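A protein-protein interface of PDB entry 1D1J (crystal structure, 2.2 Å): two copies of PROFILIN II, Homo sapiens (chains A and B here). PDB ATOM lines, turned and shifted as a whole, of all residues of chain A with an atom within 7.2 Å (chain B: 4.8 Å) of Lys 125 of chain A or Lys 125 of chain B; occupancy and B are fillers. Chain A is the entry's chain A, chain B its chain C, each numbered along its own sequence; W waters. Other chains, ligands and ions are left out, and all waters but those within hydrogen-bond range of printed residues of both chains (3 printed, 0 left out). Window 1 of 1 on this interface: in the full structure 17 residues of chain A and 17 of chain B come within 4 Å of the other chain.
The side-chain carboxylate of Asp 86 of chain A is in hydrogen-bond range of the side-chain amide nitrogen of Asn 124 of chain A (2.8 Å). OG1 of Thr 84 of chain B is in hydrogen-bond range of OD1 of Asp 82 of chain B (2.7 Å). O of Thr 84 of chain A is in hydrogen-bond range of N of Ser 76 of chain A, at 2.8 Å. The backbone carbonyl oxygen (O) of Ser 76 of chain A lies within hydrogen-bond range of the backbone NH (N) of Cys 83 of chain A (3.3 Å). The backbone NH (N) of Asp 86 of chain A lies within hydrogen-bond range of the backbone carbonyl oxygen (O) of Arg 74 of chain A (2.9 Å). The side-chain hydroxyl (OG1) of Thr 84 of chain B sits at hydrogen-bond distance from the side-chain amide nitrogen (ND2) of Asn 124 of chain B.
Of the printed residues of chain B, Asp 80 of chain A touches Thr 122 (2.8 Å). Ala 101 of chain A touches none of the printed residues of chain B. Of the printed residues of chain B, Gly 121 of chain A touches Asp 82 (3.0 Å). Thr 122 of chain A touches none of the printed residues of chain B. Of the printed residues of chain B, Asn 124 of chain A touches Lys 125 (2.9 Å). Lys 125 of chain A touches just these residues of chain B: Gly 81, Asp 82, Thr 84, Asn 124, Lys 125 and Tyr 128. Of the printed residues of chain A, Asn 124 of chain B touches Lys 125 (2.8 Å). Of chain A, only Gly 81, Asp 82, Thr 84, Asn 124, Lys 125 and Tyr 128 come within 4 Å of Lys 125 of chain B. Printed residues of chain A within 4 Å of Glu 129 of chain B: Tyr 128 (2.8 Å). The nearest printed residue of chain B that does not touch Lys 125 of chain A is Glu 129 of chain B (7.0 Å). The nearest residue of chain A that does not touch Lys 125 of chain B is Ser 76 of chain A (5.7 Å).
CA of Gly 121 of chain B touches OG of Ser 76 of chain A, at 3.5 Å. Gly 81 of chain A touches Lys 125 of chain B (O to CB, 3.2 Å). Lys 125 of chain B touches Thr 84 of chain A (NZ to OG1, 3.8 Å). CB of Lys 125 of chain A touches O of Gly 81 of chain B (3.3 Å). NZ of Lys 125 of chain A touches OG1 of Thr 84 of chain B (3.9 Å). Lys 125 of chain A touches Lys 125 of chain B. Lys 125 of chain A touches Tyr 128 of chain B. Tyr 128 of chain A touches Lys 125 of chain B (CD1 to CE, 3.4 Å). CE2 of Tyr 128 of chain A touches CE2 of Tyr 128 of chain B, 3.8 Å away.
Among the printed residues, Asp or Glu carboxylates within 4 Å of a Lys or Arg side-chain nitrogen of the other chain: Asp 82 of chain A with Lys 125 of chain B and Lys 125 of chain A with Asp 82 of chain B.
Asp 82 of chain A touches Gly 121 of chain B, and with the chains exchanged Gly 121 of chain A touches Asp 82 of chain B. Asp 82 of chain A touches Lys 125 of chain B, and with the chains exchanged Lys 125 of chain A touches Asp 82 of chain B. Thr 84 of chain A touches Lys 125 of chain B, and with the chains exchanged Lys 125 of chain A touches Thr 84 of chain B. Lys 125 of chain A touches its own counterpart, Lys 125 of chain B. 12 positions are printed for both chains. Of the 19 pairs that touch across the chains among the printed residues, 16 have their exchanged pair printed and touching as well.
The side-chain hydroxyl (OG1) of Thr 122 of chain B lies within hydrogen-bond range of the backbone carbonyl oxygen (O) of Asp 80 of chain A (2.8 Å). OD2 of Asp 82 of chain A lies close to O of Gly 121 of chain B (3.0 Å). NH1 of Arg 74 of chain A lies close to N of Gly 121 of chain B (3.5 Å). OH of Tyr 128 of chain A lies within hydrogen-bond range of OE2 of Glu 129 of chain B (2.8 Å). O of Gly 121 of chain A lies close to OD2 of Asp 82 of chain B (3.0 Å). The side-chain carboxylate of Glu 129 of chain A lies within hydrogen-bond range of the side-chain hydroxyl of Tyr 128 of chain B (2.7 Å). The side-chain amide oxygen (OD1) of Asn 124 of chain A sits at hydrogen-bond distance from the side-chain amino group (NZ) of Lys 125 of chain B, 2.9 Å away. The side-chain amino group of Lys 125 of chain A sits at hydrogen-bond distance from the side-chain amide oxygen of Asn 124 of chain B (2.8 Å). The side-chain amino group (NZ) of Lys 125 of chain B lies within salt-bridge range of the side-chain carboxylate (OD2) of Asp 82 of chain A. The side-chain amino group of Lys 125 of chain A lies within salt-bridge range of the side-chain carboxylate of Asp 82 of chain B (2.9 Å).
Water W3 bridges the side-chain hydroxyl (OG) of Ser 76 of chain A (2.7 Å) and the backbone NH (N) of Gly 121 of chain B (2.9 Å). Water W1 bridges the side-chain amino group (NZ) of Lys 125 of chain A (2.9 Å) and the side-chain carboxylate (OD2) of Asp 82 of chain B (3.1 Å). Water W2 lies within hydrogen-bond range of NZ of Lys 125 of chain B, OD2 of Asp 82 of chain A and OD1 of Asn 124 of chain B.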
ATOM      1  N   ARG A  74      -1.074   8.720  13.747  1.00  0.00           N
ATOM      2  CA  ARG A  74      -2.470   8.306  13.823  1.00  0.00           C
ATOM      3  C   ARG A  74      -2.716   6.958  13.153  1.00  0.00           C
ATOM      4  O   ARG A  74      -2.121   6.648  12.120  1.00  0.00           O
ATOM      5  CB  ARG A  74      -3.399   9.361  13.196  1.00  0.00           C
ATOM      6  CG  ARG A  74      -4.824   8.834  12.942  1.00  0.00           C
ATOM      7  CD  ARG A  74      -5.785   9.905  12.487  1.00  0.00           C
ATOM      8  NE  ARG A  74      -5.924  10.926  13.515  1.00  0.00           N
ATOM      9  CZ  ARG A  74      -6.855  11.871  13.515  1.00  0.00           C
ATOM     10  NH1 ARG A  74      -7.756  11.924  12.536  1.00  0.00           N
ATOM     11  NH2 ARG A  74      -6.839  12.806  14.462  1.00  0.00           N
ATOM     12  N   SER A  76      -5.672   4.763  11.474  1.00  0.00           N
ATOM     13  CA  SER A  76      -7.021   4.734  10.898  1.00  0.00           C
ATOM     14  C   SER A  76      -7.096   3.568   9.914  1.00  0.00           C
ATOM     15  O   SER A  76      -7.979   3.518   9.063  1.00  0.00           O
ATOM     16  CB  SER A  76      -7.308   6.031  10.123  1.00  0.00           C
ATOM     17  OG  SER A  76      -7.050   7.188  10.893  1.00  0.00           O
ATOM     18  N   ASP A  80     -13.673   2.705  10.699  1.00  0.00           N
ATOM     19  CA  ASP A  80     -14.760   2.954   9.753  1.00  0.00           C
ATOM     20  C   ASP A  80     -14.490   4.128   8.807  1.00  0.00           C
ATOM     21  O   ASP A  80     -14.043   5.193   9.231  1.00  0.00           O
ATOM     22  CB  ASP A  80     -16.083   3.198  10.506  1.00  0.00           C
ATOM     23  CG  ASP A  80     -16.607   1.942  11.245  1.00  0.00           C
ATOM     24  OD1 ASP A  80     -16.057   0.832  11.054  1.00  0.00           O
ATOM     25  OD2 ASP A  80     -17.584   2.081  12.015  1.00  0.00           O
ATOM     26  N   GLY A  81     -14.737   3.917   7.519  1.00  0.00           N
ATOM     27  CA  GLY A  81     -14.541   4.977   6.543  1.00  0.00           C
ATOM     28  C   GLY A  81     -13.119   5.424   6.234  1.00  0.00           C
ATOM     29  O   GLY A  81     -12.931   6.369   5.466  1.00  0.00           O
ATOM     30  N   ASP A  82     -12.121   4.771   6.828  1.00  0.00           N
ATOM     31  CA  ASP A  82     -10.722   5.121   6.574  1.00  0.00           C
ATOM     32  C   ASP A  82      -9.881   3.841   6.354  1.00  0.00           C
ATOM     33  O   ASP A  82     -10.369   2.730   6.547  1.00  0.00           O
ATOM     34  CB  ASP A  82     -10.174   5.953   7.741  1.00  0.00           C
ATOM     35  CG  ASP A  82      -9.074   6.921   7.320  1.00  0.00           C
ATOM     36  OD1 ASP A  82      -8.328   6.624   6.378  1.00  0.00           O
ATOM     37  OD2 ASP A  82      -8.953   7.996   7.938  1.00  0.00           O
ATOM     38  N   CYS A  83      -8.635   4.004   5.917  1.00  0.00           N
ATOM     39  CA  CYS A  83      -7.743   2.880   5.660  1.00  0.00           C
ATOM     40  C   CYS A  83      -6.303   3.370   5.663  1.00  0.00           C
ATOM     41  O   CYS A  83      -5.437   2.777   5.023  1.00  0.00           O
ATOM     42  CB  CYS A  83      -8.063   2.275   4.288  1.00  0.00           C
ATOM     43  SG  CYS A  83      -7.808   3.403   2.877  1.00  0.00           S
ATOM     44  N   THR A  84      -6.039   4.425   6.425  1.00  0.00           N
ATOM     45  CA  THR A  84      -4.700   5.020   6.464  1.00  0.00           C
ATOM     46  C   THR A  84      -4.043   5.053   7.839  1.00  0.00           C
ATOM     47  O   THR A  84      -4.698   4.901   8.865  1.00  0.00           O
ATOM     48  CB  THR A  84      -4.732   6.492   5.947  1.00  0.00           C
ATOM     49  OG1 THR A  84      -5.662   7.244   6.736  1.00  0.00           O
ATOM     50  CG2 THR A  84      -5.144   6.562   4.471  1.00  0.00           C
ATOM     51  N   ASP A  86      -0.843   7.468   9.676  1.00  0.00           N
ATOM     52  CA  ASP A  86       0.069   8.593   9.527  1.00  0.00           C
ATOM     53  C   ASP A  86       1.296   8.324  10.369  1.00  0.00           C
ATOM     54  O   ASP A  86       1.214   8.226  11.585  1.00  0.00           O
ATOM     55  CB  ASP A  86      -0.630   9.884   9.936  1.00  0.00           C
ATOM     56  CG  ASP A  86      -1.892  10.116   9.136  1.00  0.00           C
ATOM     57  OD1 ASP A  86      -1.796  10.093   7.888  1.00  0.00           O
ATOM     58  OD2 ASP A  86      -2.976  10.276   9.744  1.00  0.00           O
ATOM     59  N   ALA A 101       2.870   7.784   4.863  1.00  0.00           N
ATOM     60  CA  ALA A 101       1.457   7.414   4.911  1.00  0.00           C
ATOM     61  C   ALA A 101       1.269   5.988   4.409  1.00  0.00           C
ATOM     62  O   ALA A 101       1.996   5.530   3.520  1.00  0.00           O
ATOM     63  CB  ALA A 101       0.586   8.388   4.104  1.00  0.00           C
ATOM     64  N   GLY A 120       1.702  15.692   6.366  1.00  0.00           N
ATOM     65  CA  GLY A 120       1.068  14.385   6.483  1.00  0.00           C
ATOM     66  C   GLY A 120      -0.279  14.308   5.780  1.00  0.00           C
ATOM     67  O   GLY A 120      -0.597  13.281   5.192  1.00  0.00           O
ATOM     68  N   GLY A 121      -1.055  15.396   5.835  1.00  0.00           N
ATOM     69  CA  GLY A 121      -2.354  15.446   5.186  1.00  0.00           C
ATOM     70  C   GLY A 121      -2.240  15.170   3.700  1.00  0.00           C
ATOM     71  O   GLY A 121      -3.071  14.464   3.128  1.00  0.00           O
ATOM     72  N   THR A 122      -1.197  15.723   3.080  1.00  0.00           N
ATOM     73  CA  THR A 122      -0.919  15.536   1.652  1.00  0.00           C
ATOM     74  C   THR A 122      -0.722  14.048   1.349  1.00  0.00           C
ATOM     75  O   THR A 122      -1.338  13.509   0.427  1.00  0.00           O
ATOM     76  CB  THR A 122       0.385  16.286   1.218  1.00  0.00           C
ATOM     77  OG1 THR A 122       0.238  17.693   1.446  1.00  0.00           O
ATOM     78  CG2 THR A 122       0.699  16.046  -0.253  1.00  0.00           C
ATOM     79  N   LEU A 123       0.138  13.408   2.144  1.00  0.00           N
ATOM     80  CA  LEU A 123       0.470  11.990   1.994  1.00  0.00           C
ATOM     81  C   LEU A 123      -0.679  11.066   2.386  1.00  0.00           C
ATOM     82  O   LEU A 123      -0.853  10.001   1.789  1.00  0.00           O
ATOM     83  CB  LEU A 123       1.724  11.647   2.813  1.00  0.00           C
ATOM     84  CG  LEU A 123       2.973  12.454   2.451  1.00  0.00           C
ATOM     85  CD1 LEU A 123       4.052  12.260   3.492  1.00  0.00           C
ATOM     86  CD2 LEU A 123       3.470  12.078   1.058  1.00  0.00           C
ATOM     87  N   ASN A 124      -1.444  11.481   3.394  1.00  0.00           N
ATOM     88  CA  ASN A 124      -2.593  10.723   3.888  1.00  0.00           C
ATOM     89  C   ASN A 124      -3.620  10.565   2.766  1.00  0.00           C
ATOM     90  O   ASN A 124      -4.129   9.465   2.532  1.00  0.00           O
ATOM     91  CB  ASN A 124      -3.211  11.448   5.091  1.00  0.00           C
ATOM     92  CG  ASN A 124      -4.470  10.782   5.607  1.00  0.00           C
ATOM     93  OD1 ASN A 124      -5.557  10.975   5.071  1.00  0.00           O
ATOM     94  ND2 ASN A 124      -4.329  10.009   6.663  1.00  0.00           N
ATOM     95  N   LYS A 125      -3.891  11.661   2.056  1.00  0.00           N
ATOM     96  CA  LYS A 125      -4.854  11.651   0.962  1.00  0.00           C
ATOM     97  C   LYS A 125      -4.265  11.025  -0.299  1.00  0.00           C
ATOM     98  O   LYS A 125      -4.999  10.509  -1.146  1.00  0.00           O
ATOM     99  CB  LYS A 125      -5.386  13.059   0.679  1.00  0.00           C
ATOM    100  CG  LYS A 125      -6.140  13.679   1.846  1.00  0.00           C
ATOM    101  CD  LYS A 125      -7.262  12.786   2.324  1.00  0.00           C
ATOM    102  CE  LYS A 125      -7.979  13.405   3.509  1.00  0.00           C
ATOM    103  NZ  LYS A 125      -7.107  13.507   4.708  1.00  0.00           N
ATOM    104  N   LYS A 126      -2.939  11.061  -0.414  1.00  0.00           N
ATOM    105  CA  LYS A 126      -2.251  10.460  -1.558  1.00  0.00           C
ATOM    106  C   LYS A 126      -2.415   8.927  -1.462  1.00  0.00           C
ATOM    107  O   LYS A 126      -2.779   8.260  -2.436  1.00  0.00           O
ATOM    108  CB  LYS A 126      -0.773  10.837  -1.526  1.00  0.00           C
ATOM    109  CG  LYS A 126       0.007  10.392  -2.731  1.00  0.00           C
ATOM    110  CD  LYS A 126       1.440  10.883  -2.633  1.00  0.00           C
ATOM    111  CE  LYS A 126       2.184  10.581  -3.913  1.00  0.00           C
ATOM    112  NZ  LYS A 126       1.480  11.154  -5.107  1.00  0.00           N
ATOM    113  N   ALA A 127      -2.149   8.388  -0.272  1.00  0.00           N
ATOM    114  CA  ALA A 127      -2.287   6.961  -0.011  1.00  0.00           C
ATOM    115  C   ALA A 127      -3.783   6.605  -0.062  1.00  0.00           C
ATOM    116  O   ALA A 127      -4.174   5.643  -0.716  1.00  0.00           O
ATOM    117  CB  ALA A 127      -1.708   6.630   1.355  1.00  0.00           C
ATOM    118  N   TYR A 128      -4.607   7.427   0.595  1.00  0.00           N
ATOM    119  CA  TYR A 128      -6.056   7.233   0.635  1.00  0.00           C
ATOM    120  C   TYR A 128      -6.648   7.143  -0.763  1.00  0.00           C
ATOM    121  O   TYR A 128      -7.411   6.222  -1.055  1.00  0.00           O
ATOM    122  CB  TYR A 128      -6.738   8.372   1.397  1.00  0.00           C
ATOM    123  CG  TYR A 128      -8.250   8.273   1.408  1.00  0.00           C
ATOM    124  CD1 TYR A 128      -8.907   7.371   2.259  1.00  0.00           C
ATOM    125  CD2 TYR A 128      -9.028   9.081   0.575  1.00  0.00           C
ATOM    126  CE1 TYR A 128     -10.294   7.283   2.281  1.00  0.00           C
ATOM    127  CE2 TYR A 128     -10.419   9.001   0.585  1.00  0.00           C
ATOM    128  CZ  TYR A 128     -11.045   8.101   1.440  1.00  0.00           C
ATOM    129  OH  TYR A 128     -12.415   8.021   1.461  1.00  0.00           O
ATOM    130  N   GLU A 129      -6.298   8.095  -1.623  1.00  0.00           N
ATOM    131  CA  GLU A 129      -6.812   8.099  -2.992  1.00  0.00           C
ATOM    132  C   GLU A 129      -6.458   6.841  -3.795  1.00  0.00           C
ATOM    133  O   GLU A 129      -7.334   6.269  -4.438  1.00  0.00           O
ATOM    134  CB  GLU A 129      -6.387   9.363  -3.760  1.00  0.00           C
ATOM    135  CG  GLU A 129      -7.124  10.649  -3.343  1.00  0.00           C
ATOM    136  CD  GLU A 129      -8.642  10.570  -3.522  1.00  0.00           C
ATOM    137  OE1 GLU A 129      -9.115   9.896  -4.463  1.00  0.00           O
ATOM    138  OE2 GLU A 129      -9.364  11.198  -2.721  1.00  0.00           O
ATOM    139  N   LEU A 130      -5.204   6.394  -3.747  1.00  0.00           N
ATOM    140  CA  LEU A 130      -4.820   5.199  -4.499  1.00  0.00           C
ATOM    141  C   LEU A 130      -5.480   3.936  -3.947  1.00  0.00           C
ATOM    142  O   LEU A 130      -5.838   3.041  -4.713  1.00  0.00           O
ATOM    143  CB  LEU A 130      -3.302   5.016  -4.553  1.00  0.00           C
ATOM    144  CG  LEU A 130      -2.879   3.841  -5.447  1.00  0.00           C
ATOM    145  CD1 LEU A 130      -3.420   4.044  -6.869  1.00  0.00           C
ATOM    146  CD2 LEU A 130      -1.360   3.684  -5.455  1.00  0.00           C
ATOM    147  N   ALA A 131      -5.621   3.867  -2.624  1.00  0.00           N
ATOM    148  CA  ALA A 131      -6.260   2.729  -1.958  1.00  0.00           C
ATOM    149  C   ALA A 131      -7.739   2.663  -2.359  1.00  0.00           C
ATOM    150  O   ALA A 131      -8.254   1.588  -2.674  1.00  0.00           O
ATOM    151  CB  ALA A 131      -6.129   2.851  -0.437  1.00  0.00           C
ATOM    152  N   GLY B  81      -3.288  18.612  -1.808  1.00  0.00           N
ATOM    153  CA  GLY B  81      -4.031  17.363  -1.790  1.00  0.00           C
ATOM    154  C   GLY B  81      -5.021  17.111  -0.661  1.00  0.00           C
ATOM    155  O   GLY B  81      -5.667  16.065  -0.656  1.00  0.00           O
ATOM    156  N   ASP B  82      -5.137  18.037   0.292  1.00  0.00           N
ATOM    157  CA  ASP B  82      -6.075  17.878   1.403  1.00  0.00           C
ATOM    158  C   ASP B  82      -6.901  19.148   1.552  1.00  0.00           C
ATOM    159  O   ASP B  82      -6.663  20.140   0.862  1.00  0.00           O
ATOM    160  CB  ASP B  82      -5.327  17.595   2.712  1.00  0.00           C
ATOM    161  CG  ASP B  82      -6.095  16.654   3.655  1.00  0.00           C
ATOM    162  OD1 ASP B  82      -7.336  16.737   3.777  1.00  0.00           O
ATOM    163  OD2 ASP B  82      -5.433  15.824   4.295  1.00  0.00           O
ATOM    164  N   THR B  84      -8.775  19.381   4.995  1.00  0.00           N
ATOM    165  CA  THR B  84      -9.358  19.054   6.303  1.00  0.00           C
ATOM    166  C   THR B  84      -8.615  19.552   7.549  1.00  0.00           C
ATOM    167  O   THR B  84      -7.455  19.946   7.496  1.00  0.00           O
ATOM    168  CB  THR B  84      -9.506  17.518   6.479  1.00  0.00           C
ATOM    169  OG1 THR B  84      -8.219  16.904   6.303  1.00  0.00           O
ATOM    170  CG2 THR B  84     -10.509  16.924   5.473  1.00  0.00           C
ATOM    171  N   GLY B 121     -10.125   9.425  12.092  1.00  0.00           N
ATOM    172  CA  GLY B 121     -10.004   9.030  10.693  1.00  0.00           C
ATOM    173  C   GLY B 121     -11.351   8.907   9.984  1.00  0.00           C
ATOM    174  O   GLY B 121     -11.500   9.282   8.821  1.00  0.00           O
ATOM    175  N   THR B 122     -12.335   8.368  10.699  1.00  0.00           N
ATOM    176  CA  THR B 122     -13.703   8.201  10.194  1.00  0.00           C
ATOM    177  C   THR B 122     -14.309   9.573   9.862  1.00  0.00           C
ATOM    178  O   THR B 122     -14.919   9.770   8.812  1.00  0.00           O
ATOM    179  CB  THR B 122     -14.599   7.534  11.278  1.00  0.00           C
ATOM    180  OG1 THR B 122     -13.957   6.355  11.783  1.00  0.00           O
ATOM    181  CG2 THR B 122     -15.961   7.178  10.714  1.00  0.00           C
ATOM    182  N   LEU B 123     -14.143  10.513  10.783  1.00  0.00           N
ATOM    183  CA  LEU B 123     -14.672  11.864  10.599  1.00  0.00           C
ATOM    184  C   LEU B 123     -13.890  12.627   9.521  1.00  0.00           C
ATOM    185  O   LEU B 123     -14.475  13.322   8.689  1.00  0.00           O
ATOM    186  CB  LEU B 123     -14.657  12.620  11.936  1.00  0.00           C
ATOM    187  CG  LEU B 123     -15.428  11.973  13.099  1.00  0.00           C
ATOM    188  CD1 LEU B 123     -15.236  12.796  14.343  1.00  0.00           C
ATOM    189  CD2 LEU B 123     -16.906  11.823  12.791  1.00  0.00           C
ATOM    190  N   ASN B 124     -12.572  12.429   9.505  1.00  0.00           N
ATOM    191  CA  ASN B 124     -11.687  13.083   8.548  1.00  0.00           C
ATOM    192  C   ASN B 124     -12.125  12.753   7.137  1.00  0.00           C
ATOM    193  O   ASN B 124     -12.349  13.648   6.324  1.00  0.00           O
ATOM    194  CB  ASN B 124     -10.235  12.634   8.755  1.00  0.00           C
ATOM    195  CG  ASN B 124      -9.270  13.292   7.777  1.00  0.00           C
ATOM    196  OD1 ASN B 124      -8.942  12.728   6.733  1.00  0.00           O
ATOM    197  ND2 ASN B 124      -8.825  14.498   8.106  1.00  0.00           N
ATOM    198  N   LYS B 125     -12.306  11.462   6.866  1.00  0.00           N
ATOM    199  CA  LYS B 125     -12.713  11.028   5.536  1.00  0.00           C
ATOM    200  C   LYS B 125     -14.150  11.374   5.185  1.00  0.00           C
ATOM    201  O   LYS B 125     -14.462  11.591   4.012  1.00  0.00           O
ATOM    202  CB  LYS B 125     -12.424   9.546   5.342  1.00  0.00           C
ATOM    203  CG  LYS B 125     -10.938   9.236   5.455  1.00  0.00           C
ATOM    204  CD  LYS B 125     -10.070  10.046   4.478  1.00  0.00           C
ATOM    205  CE  LYS B 125      -8.576   9.752   4.686  1.00  0.00           C
ATOM    206  NZ  LYS B 125      -8.117  10.026   6.090  1.00  0.00           N
ATOM    207  N   LYS B 126     -15.022  11.420   6.194  1.00  0.00           N
ATOM    208  CA  LYS B 126     -16.419  11.782   5.977  1.00  0.00           C
ATOM    209  C   LYS B 126     -16.466  13.252   5.525  1.00  0.00           C
ATOM    210  O   LYS B 126     -17.169  13.600   4.570  1.00  0.00           O
ATOM    211  CB  LYS B 126     -17.235  11.619   7.269  1.00  0.00           C
ATOM    212  CG  LYS B 126     -18.666  12.161   7.160  1.00  0.00           C
ATOM    213  CD  LYS B 126     -19.400  12.159   8.497  1.00  0.00           C
ATOM    214  CE  LYS B 126     -19.721  10.751   8.946  1.00  0.00           C
ATOM    215  NZ  LYS B 126     -20.645  10.092   7.990  1.00  0.00           N
ATOM    216  N   ALA B 127     -15.715  14.098   6.238  1.00  0.00           N
ATOM    217  CA  ALA B 127     -15.623  15.534   5.956  1.00  0.00           C
ATOM    218  C   ALA B 127     -14.992  15.771   4.585  1.00  0.00           C
ATOM    219  O   ALA B 127     -15.482  16.590   3.799  1.00  0.00           O
ATOM    220  CB  ALA B 127     -14.800  16.229   7.029  1.00  0.00           C
ATOM    221  N   TYR B 128     -13.935  15.002   4.306  1.00  0.00           N
ATOM    222  CA  TYR B 128     -13.189  15.067   3.050  1.00  0.00           C
ATOM    223  C   TYR B 128     -14.052  14.728   1.848  1.00  0.00           C
ATOM    224  O   TYR B 128     -14.079  15.491   0.881  1.00  0.00           O
ATOM    225  CB  TYR B 128     -11.967  14.134   3.116  1.00  0.00           C
ATOM    226  CG  TYR B 128     -11.150  14.010   1.841  1.00  0.00           C
ATOM    227  CD1 TYR B 128     -10.240  15.004   1.460  1.00  0.00           C
ATOM    228  CD2 TYR B 128     -11.239  12.863   1.050  1.00  0.00           C
ATOM    229  CE1 TYR B 128      -9.433  14.848   0.326  1.00  0.00           C
ATOM    230  CE2 TYR B 128     -10.453  12.701  -0.074  1.00  0.00           C
ATOM    231  CZ  TYR B 128      -9.545  13.694  -0.440  1.00  0.00           C
ATOM    232  OH  TYR B 128      -8.777  13.525  -1.580  1.00  0.00           O
ATOM    233  N   GLU B 129     -14.786  13.619   1.924  1.00  0.00           N
ATOM    234  CA  GLU B 129     -15.641  13.183   0.819  1.00  0.00           C
ATOM    235  C   GLU B 129     -16.741  14.164   0.445  1.00  0.00           C
ATOM    236  O   GLU B 129     -16.997  14.381  -0.740  1.00  0.00           O
ATOM    237  CB  GLU B 129     -16.255  11.796   1.095  1.00  0.00           C
ATOM    238  CG  GLU B 129     -15.271  10.615   1.068  1.00  0.00           C
ATOM    239  CD  GLU B 129     -14.645  10.364  -0.306  1.00  0.00           C
ATOM    240  OE1 GLU B 129     -15.218  10.796  -1.323  1.00  0.00           O
ATOM    241  OE2 GLU B 129     -13.586   9.712  -0.378  1.00  0.00           O
HETATM  242  O   HOH W   1      -5.246  14.076   6.883  1.00  0.00           O
HETATM  243  O   HOH W   2      -7.265  10.625   8.914  1.00  0.00           O
HETATM  244  O   HOH W   3      -8.304   7.499  13.279  1.00  0.00           O
